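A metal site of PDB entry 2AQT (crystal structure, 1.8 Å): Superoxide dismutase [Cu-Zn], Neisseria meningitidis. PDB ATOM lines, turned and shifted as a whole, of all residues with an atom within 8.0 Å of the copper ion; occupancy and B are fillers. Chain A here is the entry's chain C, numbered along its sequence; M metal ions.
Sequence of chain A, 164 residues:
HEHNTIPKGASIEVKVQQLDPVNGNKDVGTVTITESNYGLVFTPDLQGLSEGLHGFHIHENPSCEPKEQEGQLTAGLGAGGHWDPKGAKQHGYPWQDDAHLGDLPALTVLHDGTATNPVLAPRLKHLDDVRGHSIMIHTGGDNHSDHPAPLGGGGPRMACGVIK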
ATOM      1  N   GLY A  55     -33.455 -13.899  -5.362  1.00  0.00           N
ATOM      2  CA  GLY A  55     -32.854 -12.987  -6.323  1.00  0.00           C
ATOM      3  C   GLY A  55     -31.349 -13.126  -6.192  1.00  0.00           C
ATOM      4  O   GLY A  55     -30.821 -13.135  -5.081  1.00  0.00           O
ATOM      5  N   PHE A  56     -30.679 -13.201  -7.334  1.00  0.00           N
ATOM      6  CA  PHE A  56     -29.234 -13.419  -7.377  1.00  0.00           C
ATOM      7  C   PHE A  56     -28.623 -12.490  -8.448  1.00  0.00           C
ATOM      8  O   PHE A  56     -28.830 -12.703  -9.635  1.00  0.00           O
ATOM      9  CB  PHE A  56     -29.042 -14.893  -7.732  1.00  0.00           C
ATOM     10  CG  PHE A  56     -27.649 -15.420  -7.538  1.00  0.00           C
ATOM     11  CD1 PHE A  56     -26.908 -15.073  -6.413  1.00  0.00           C
ATOM     12  CD2 PHE A  56     -27.124 -16.348  -8.429  1.00  0.00           C
ATOM     13  CE1 PHE A  56     -25.668 -15.662  -6.175  1.00  0.00           C
ATOM     14  CE2 PHE A  56     -25.896 -16.937  -8.210  1.00  0.00           C
ATOM     15  CZ  PHE A  56     -25.157 -16.602  -7.079  1.00  0.00           C
ATOM     16  N   HIS A  57     -27.889 -11.457  -8.016  1.00  0.00           N
ATOM     17  CA  HIS A  57     -27.297 -10.517  -8.973  1.00  0.00           C
ATOM     18  C   HIS A  57     -25.889 -10.061  -8.630  1.00  0.00           C
ATOM     19  O   HIS A  57     -25.441 -10.150  -7.486  1.00  0.00           O
ATOM     20  CB  HIS A  57     -28.145  -9.239  -9.091  1.00  0.00           C
ATOM     21  CG  HIS A  57     -29.609  -9.443  -8.840  1.00  0.00           C
ATOM     22  ND1 HIS A  57     -30.240  -8.943  -7.722  1.00  0.00           N
ATOM     23  CD2 HIS A  57     -30.562 -10.071  -9.574  1.00  0.00           C
ATOM     24  CE1 HIS A  57     -31.521  -9.264  -7.771  1.00  0.00           C
ATOM     25  NE2 HIS A  57     -31.746  -9.943  -8.884  1.00  0.00           N
ATOM     26  N   ILE A  58     -25.191  -9.576  -9.640  1.00  0.00           N
ATOM     27  CA  ILE A  58     -23.865  -9.012  -9.425  1.00  0.00           C
ATOM     28  C   ILE A  58     -24.144  -7.520  -9.252  1.00  0.00           C
ATOM     29  O   ILE A  58     -24.824  -6.919 -10.088  1.00  0.00           O
ATOM     30  CB  ILE A  58     -22.940  -9.200 -10.651  1.00  0.00           C
ATOM     31  CG1 ILE A  58     -22.730 -10.687 -10.939  1.00  0.00           C
ATOM     32  CG2 ILE A  58     -21.602  -8.511 -10.401  1.00  0.00           C
ATOM     33  CD1 ILE A  58     -22.131 -11.449  -9.777  1.00  0.00           C
ATOM     34  N   HIS A  59     -23.646  -6.935  -8.169  1.00  0.00           N
ATOM     35  CA  HIS A  59     -23.845  -5.511  -7.931  1.00  0.00           C
ATOM     36  C   HIS A  59     -22.596  -4.718  -8.278  1.00  0.00           C
ATOM     37  O   HIS A  59     -21.474  -5.248  -8.279  1.00  0.00           O
ATOM     38  CB  HIS A  59     -24.295  -5.276  -6.477  1.00  0.00           C
ATOM     39  CG  HIS A  59     -25.737  -5.585  -6.245  1.00  0.00           C
ATOM     40  ND1 HIS A  59     -26.631  -4.663  -5.746  1.00  0.00           N
ATOM     41  CD2 HIS A  59     -26.460  -6.703  -6.489  1.00  0.00           C
ATOM     42  CE1 HIS A  59     -27.839  -5.196  -5.695  1.00  0.00           C
ATOM     43  NE2 HIS A  59     -27.765  -6.429  -6.147  1.00  0.00           N
ATOM     44  N   ALA A  79     -22.940  -2.024  -1.707  1.00  0.00           N
ATOM     45  CA  ALA A  79     -22.711  -2.684  -2.981  1.00  0.00           C
ATOM     46  C   ALA A  79     -23.238  -1.878  -4.170  1.00  0.00           C
ATOM     47  O   ALA A  79     -22.864  -2.134  -5.311  1.00  0.00           O
ATOM     48  CB  ALA A  79     -23.368  -4.067  -2.974  1.00  0.00           C
ATOM     49  N   GLY A  80     -24.095  -0.905  -3.900  1.00  0.00           N
ATOM     50  CA  GLY A  80     -24.647  -0.128  -4.991  1.00  0.00           C
ATOM     51  C   GLY A  80     -25.714  -0.930  -5.706  1.00  0.00           C
ATOM     52  O   GLY A  80     -26.138  -1.979  -5.227  1.00  0.00           O
ATOM     53  N   GLY A  81     -26.147  -0.454  -6.878  1.00  0.00           N
ATOM     54  CA  GLY A  81     -27.190  -1.152  -7.606  1.00  0.00           C
ATOM     55  C   GLY A  81     -26.726  -2.325  -8.442  1.00  0.00           C
ATOM     56  O   GLY A  81     -25.562  -2.748  -8.358  1.00  0.00           O
ATOM     57  N   HIS A  82     -27.626  -2.855  -9.247  1.00  0.00           N
ATOM     58  CA  HIS A  82     -27.296  -3.968 -10.123  1.00  0.00           C
ATOM     59  C   HIS A  82     -26.214  -3.523 -11.088  1.00  0.00           C
ATOM     60  O   HIS A  82     -26.306  -2.444 -11.686  1.00  0.00           O
ATOM     61  CB  HIS A  82     -28.523  -4.430 -10.904  1.00  0.00           C
ATOM     62  CG  HIS A  82     -29.577  -5.082 -10.061  1.00  0.00           C
ATOM     63  ND1 HIS A  82     -30.549  -5.901 -10.586  1.00  0.00           N
ATOM     64  CD2 HIS A  82     -29.799  -5.038  -8.720  1.00  0.00           C
ATOM     65  CE1 HIS A  82     -31.321  -6.340  -9.608  1.00  0.00           C
ATOM     66  NE2 HIS A  82     -30.892  -5.834  -8.471  1.00  0.00           N
ATOM     67  N   TRP A  83     -25.170  -4.342 -11.229  1.00  0.00           N
ATOM     68  CA  TRP A  83     -24.063  -4.034 -12.136  1.00  0.00           C
ATOM     69  C   TRP A  83     -24.622  -3.819 -13.530  1.00  0.00           C
ATOM     70  O   TRP A  83     -25.204  -4.722 -14.131  1.00  0.00           O
ATOM     71  CB  TRP A  83     -23.058  -5.191 -12.102  1.00  0.00           C
ATOM     72  CG  TRP A  83     -21.812  -4.941 -12.890  1.00  0.00           C
ATOM     73  CD1 TRP A  83     -21.081  -3.784 -12.935  1.00  0.00           C
ATOM     74  CD2 TRP A  83     -21.116  -5.893 -13.682  1.00  0.00           C
ATOM     75  NE1 TRP A  83     -19.969  -3.962 -13.723  1.00  0.00           N
ATOM     76  CE2 TRP A  83     -19.964  -5.254 -14.200  1.00  0.00           C
ATOM     77  CE3 TRP A  83     -21.356  -7.234 -14.023  1.00  0.00           C
ATOM     78  CZ2 TRP A  83     -19.039  -5.904 -15.022  1.00  0.00           C
ATOM     79  CZ3 TRP A  83     -20.431  -7.884 -14.845  1.00  0.00           C
ATOM     80  CH2 TRP A  83     -19.289  -7.220 -15.337  1.00  0.00           C
ATOM     81  N   HIS A  91     -34.129  -4.061 -15.283  1.00  0.00           N
ATOM     82  CA  HIS A  91     -33.897  -5.410 -14.805  1.00  0.00           C
ATOM     83  C   HIS A  91     -34.543  -6.415 -15.747  1.00  0.00           C
ATOM     84  O   HIS A  91     -35.644  -6.169 -16.262  1.00  0.00           O
ATOM     85  CB  HIS A  91     -34.462  -5.571 -13.390  1.00  0.00           C
ATOM     86  CG  HIS A  91     -34.159  -6.896 -12.774  1.00  0.00           C
ATOM     87  ND1 HIS A  91     -32.885  -7.272 -12.399  1.00  0.00           N
ATOM     88  CD2 HIS A  91     -34.958  -7.948 -12.482  1.00  0.00           C
ATOM     89  CE1 HIS A  91     -32.918  -8.491 -11.899  1.00  0.00           C
ATOM     90  NE2 HIS A  91     -34.160  -8.928 -11.936  1.00  0.00           N
ATOM     91  N   HIS A 100     -29.710  -5.536 -17.092  1.00  0.00           N
ATOM     92  CA  HIS A 100     -28.468  -5.320 -16.331  1.00  0.00           C
ATOM     93  C   HIS A 100     -27.539  -6.501 -16.608  1.00  0.00           C
ATOM     94  O   HIS A 100     -27.966  -7.654 -16.556  1.00  0.00           O
ATOM     95  CB  HIS A 100     -28.759  -5.295 -14.831  1.00  0.00           C
ATOM     96  CG  HIS A 100     -29.707  -4.223 -14.405  1.00  0.00           C
ATOM     97  ND1 HIS A 100     -30.674  -4.422 -13.449  1.00  0.00           N
ATOM     98  CD2 HIS A 100     -29.804  -2.913 -14.762  1.00  0.00           C
ATOM     99  CE1 HIS A 100     -31.322  -3.298 -13.221  1.00  0.00           C
ATOM    100  NE2 HIS A 100     -30.809  -2.361 -14.009  1.00  0.00           N
ATOM    101  N   GLY A 102     -25.513  -7.635 -14.742  1.00  0.00           N
ATOM    102  CA  GLY A 102     -25.400  -8.362 -13.495  1.00  0.00           C
ATOM    103  C   GLY A 102     -26.564  -9.277 -13.145  1.00  0.00           C
ATOM    104  O   GLY A 102     -26.545  -9.931 -12.105  1.00  0.00           O
ATOM    105  N   ASP A 103     -27.594  -9.314 -13.998  1.00  0.00           N
ATOM    106  CA  ASP A 103     -28.755 -10.166 -13.724  1.00  0.00           C
ATOM    107  C   ASP A 103     -28.472 -11.638 -13.962  1.00  0.00           C
ATOM    108  O   ASP A 103     -28.407 -12.103 -15.093  1.00  0.00           O
ATOM    109  CB  ASP A 103     -29.938  -9.723 -14.571  1.00  0.00           C
ATOM    110  CG  ASP A 103     -30.388  -8.316 -14.215  1.00  0.00           C
ATOM    111  OD1 ASP A 103     -30.039  -7.862 -13.108  1.00  0.00           O
ATOM    112  OD2 ASP A 103     -31.090  -7.691 -15.045  1.00  0.00           O
ATOM    113  N   SER A 134     -19.587  -7.257  -6.628  1.00  0.00           N
ATOM    114  CA  SER A 134     -20.142  -8.085  -5.563  1.00  0.00           C
ATOM    115  C   SER A 134     -21.268  -8.973  -6.060  1.00  0.00           C
ATOM    116  O   SER A 134     -21.860  -8.737  -7.127  1.00  0.00           O
ATOM    117  CB  SER A 134     -20.656  -7.185  -4.429  1.00  0.00           C
ATOM    118  OG  SER A 134     -21.600  -6.235  -4.917  1.00  0.00           O
ATOM    119  N   ILE A 135     -21.560 -10.021  -5.291  1.00  0.00           N
ATOM    120  CA  ILE A 135     -22.614 -10.954  -5.610  1.00  0.00           C
ATOM    121  C   ILE A 135     -23.619 -10.843  -4.459  1.00  0.00           C
ATOM    122  O   ILE A 135     -23.252 -10.928  -3.290  1.00  0.00           O
ATOM    123  CB  ILE A 135     -22.049 -12.397  -5.747  1.00  0.00           C
ATOM    124  CG1 ILE A 135     -23.152 -13.374  -6.161  1.00  0.00           C
ATOM    125  CG2 ILE A 135     -21.408 -12.837  -4.457  1.00  0.00           C
ATOM    126  CD1 ILE A 135     -22.607 -14.727  -6.563  1.00  0.00           C
ATOM    127  N   MET A 136     -24.887 -10.637  -4.810  1.00  0.00           N
ATOM    128  CA  MET A 136     -25.934 -10.444  -3.819  1.00  0.00           C
ATOM    129  C   MET A 136     -27.035 -11.494  -3.911  1.00  0.00           C
ATOM    130  O   MET A 136     -27.438 -11.882  -4.995  1.00  0.00           O
ATOM    131  CB  MET A 136     -26.558  -9.068  -4.021  1.00  0.00           C
ATOM    132  CG  MET A 136     -27.386  -8.561  -2.853  1.00  0.00           C
ATOM    133  SD  MET A 136     -26.299  -7.931  -1.582  1.00  0.00           S
ATOM    134  CE  MET A 136     -25.603  -6.483  -2.412  1.00  0.00           C
ATOM    135  N   ILE A 137     -27.503 -11.941  -2.745  1.00  0.00           N
ATOM    136  CA  ILE A 137     -28.608 -12.885  -2.685  1.00  0.00           C
ATOM    137  C   ILE A 137     -29.686 -12.138  -1.904  1.00  0.00           C
ATOM    138  O   ILE A 137     -29.457 -11.679  -0.786  1.00  0.00           O
ATOM    139  CB  ILE A 137     -28.231 -14.181  -1.953  1.00  0.00           C
ATOM    140  CG1 ILE A 137     -27.095 -14.883  -2.708  1.00  0.00           C
ATOM    141  CG2 ILE A 137     -29.430 -15.104  -1.872  1.00  0.00           C
ATOM    142  CD1 ILE A 137     -26.546 -16.116  -1.994  1.00  0.00           C
ATOM    143  N   HIS A 138     -30.856 -11.986  -2.505  1.00  0.00           N
ATOM    144  CA  HIS A 138     -31.952 -11.255  -1.888  1.00  0.00           C
ATOM    145  C   HIS A 138     -32.907 -12.125  -1.087  1.00  0.00           C
ATOM    146  O   HIS A 138     -32.921 -13.350  -1.237  1.00  0.00           O
ATOM    147  CB  HIS A 138     -32.723 -10.502  -2.977  1.00  0.00           C
ATOM    148  CG  HIS A 138     -31.947  -9.384  -3.592  1.00  0.00           C
ATOM    149  ND1 HIS A 138     -32.091  -8.068  -3.207  1.00  0.00           N
ATOM    150  CD2 HIS A 138     -30.983  -9.386  -4.539  1.00  0.00           C
ATOM    151  CE1 HIS A 138     -31.257  -7.313  -3.888  1.00  0.00           C
ATOM    152  NE2 HIS A 138     -30.565  -8.084  -4.710  1.00  0.00           N
ATOM    153  N   ASP A 142     -37.030 -13.516  -7.973  1.00  0.00           N
ATOM    154  CA  ASP A 142     -36.662 -12.709  -9.138  1.00  0.00           C
ATOM    155  C   ASP A 142     -37.487 -13.133 -10.351  1.00  0.00           C
ATOM    156  O   ASP A 142     -37.268 -14.225 -10.911  1.00  0.00           O
ATOM    157  CB  ASP A 142     -35.170 -12.881  -9.441  1.00  0.00           C
ATOM    158  CG  ASP A 142     -34.647 -11.832 -10.420  1.00  0.00           C
ATOM    159  OD1 ASP A 142     -35.472 -11.153 -11.053  1.00  0.00           O
ATOM    160  OD2 ASP A 142     -33.409 -11.692 -10.539  1.00  0.00           O
ATOM    161  N   LEU A 151     -36.684  -4.338  -9.728  1.00  0.00           N
ATOM    162  CA  LEU A 151     -35.565  -5.258  -9.646  1.00  0.00           C
ATOM    163  C   LEU A 151     -35.925  -6.737  -9.433  1.00  0.00           C
ATOM    164  O   LEU A 151     -35.211  -7.465  -8.750  1.00  0.00           O
ATOM    165  CB  LEU A 151     -34.629  -4.777  -8.540  1.00  0.00           C
ATOM    166  CG  LEU A 151     -34.219  -3.309  -8.713  1.00  0.00           C
ATOM    167  CD1 LEU A 151     -33.470  -2.827  -7.480  1.00  0.00           C
ATOM    168  CD2 LEU A 151     -33.362  -3.157  -9.960  1.00  0.00           C
ATOM    169  N   GLY A 154     -36.761  -8.730  -5.601  1.00  0.00           N
ATOM    170  CA  GLY A 154     -35.812  -9.307  -4.661  1.00  0.00           C
ATOM    171  C   GLY A 154     -35.925  -8.722  -3.265  1.00  0.00           C
ATOM    172  O   GLY A 154     -35.671  -9.406  -2.270  1.00  0.00           O
ATOM    173  N   GLY A 155     -36.307  -7.459  -3.180  1.00  0.00           N
ATOM    174  CA  GLY A 155     -36.438  -6.847  -1.872  1.00  0.00           C
ATOM    175  C   GLY A 155     -35.097  -6.689  -1.164  1.00  0.00           C
ATOM    176  O   GLY A 155     -34.071  -6.499  -1.829  1.00  0.00           O
ATOM    177  N   PRO A 156     -35.082  -6.774   0.175  1.00  0.00           N
ATOM    178  CA  PRO A 156     -33.881  -6.630   0.998  1.00  0.00           C
ATOM    179  C   PRO A 156     -32.709  -7.539   0.629  1.00  0.00           C
ATOM    180  O   PRO A 156     -32.886  -8.664   0.151  1.00  0.00           O
ATOM    181  CB  PRO A 156     -34.398  -6.892   2.412  1.00  0.00           C
ATOM    182  CG  PRO A 156     -35.801  -6.374   2.342  1.00  0.00           C
ATOM    183  CD  PRO A 156     -36.273  -6.952   1.021  1.00  0.00           C
ATOM    184  N   ARG A 157     -31.507  -7.037   0.881  1.00  0.00           N
ATOM    185  CA  ARG A 157     -30.270  -7.760   0.611  1.00  0.00           C
ATOM    186  C   ARG A 157     -29.981  -8.670   1.801  1.00  0.00           C
ATOM    187  O   ARG A 157     -29.662  -8.202   2.894  1.00  0.00           O
ATOM    188  CB  ARG A 157     -29.157  -6.738   0.373  1.00  0.00           C
ATOM    189  CG  ARG A 157     -29.538  -5.803  -0.745  1.00  0.00           C
ATOM    190  CD  ARG A 157     -28.507  -4.750  -1.086  1.00  0.00           C
ATOM    191  NE  ARG A 157     -29.014  -3.919  -2.169  1.00  0.00           N
ATOM    192  CZ  ARG A 157     -28.279  -3.063  -2.880  1.00  0.00           C
ATOM    193  NH1 ARG A 157     -26.985  -2.913  -2.619  1.00  0.00           N
ATOM    194  NH2 ARG A 157     -28.851  -2.361  -3.848  1.00  0.00           N
ATOM    195  N   ALA A 159     -27.825 -11.789   1.683  1.00  0.00           N
ATOM    196  CA  ALA A 159     -26.461 -12.320   1.760  1.00  0.00           C
ATOM    197  C   ALA A 159     -25.601 -11.674   0.682  1.00  0.00           C
ATOM    198  O   ALA A 159     -26.111 -11.281  -0.356  1.00  0.00           O
ATOM    199  CB  ALA A 159     -26.480 -13.839   1.599  1.00  0.00           C
HETATM  200 CU    CU M   1     -29.336  -7.763  -6.331  1.00  0.00          CU
HETATM  201 ZN    ZN M   2     -30.999  -6.257 -12.520  1.00  0.00          ZN
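A ring nitrogen (ND1) of His 59 lies close to the backbone carbonyl oxygen (O) of Gly 81 (3.4 Å). ND1 of His 138 lies within hydrogen-bond range of O of Gly 155, 2.9 Å away. The backbone carbonyl oxygen (O) of Ser 134 is in hydrogen-bond range of the backbone NH (N) of His 59 (2.7 Å). A ring nitrogen (ND1) of His 59 is in hydrogen-bond range of the backbone carbonyl oxygen of Gly 80 (2.8 Å). N of His 138 sits at hydrogen-bond distance from O of Gly 55 (2.8 Å). A ring nitrogen (NE2) of His 57 lies within hydrogen-bond range of the side-chain carboxylate of Asp 142, at 2.9 Å. The backbone carbonyl oxygen of His 57 lies within hydrogen-bond range of the backbone NH of Met 136, 2.8 Å away. A ring nitrogen (ND1) of His 57 sits close to a ring nitrogen (NE2) of His 82 (3.3 Å).
Residues that only touch the copper ion: His 82 (3.3 Å) and Met 136 (3.8 Å). Within 4 Å of the copper ion: His 57, His 59, His 82, Met 136 and His 138. The nearest printed residue that does not touch the copper ion is Phe 56 (5.2 Å).
The copper ion is bound by ND1 of His 57 (2.0 Å). A ring nitrogen (NE2) of His 138 is bound to the copper ion. A ring nitrogen (NE2) of His 59 is bound to the copper ion (2.1 Å).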
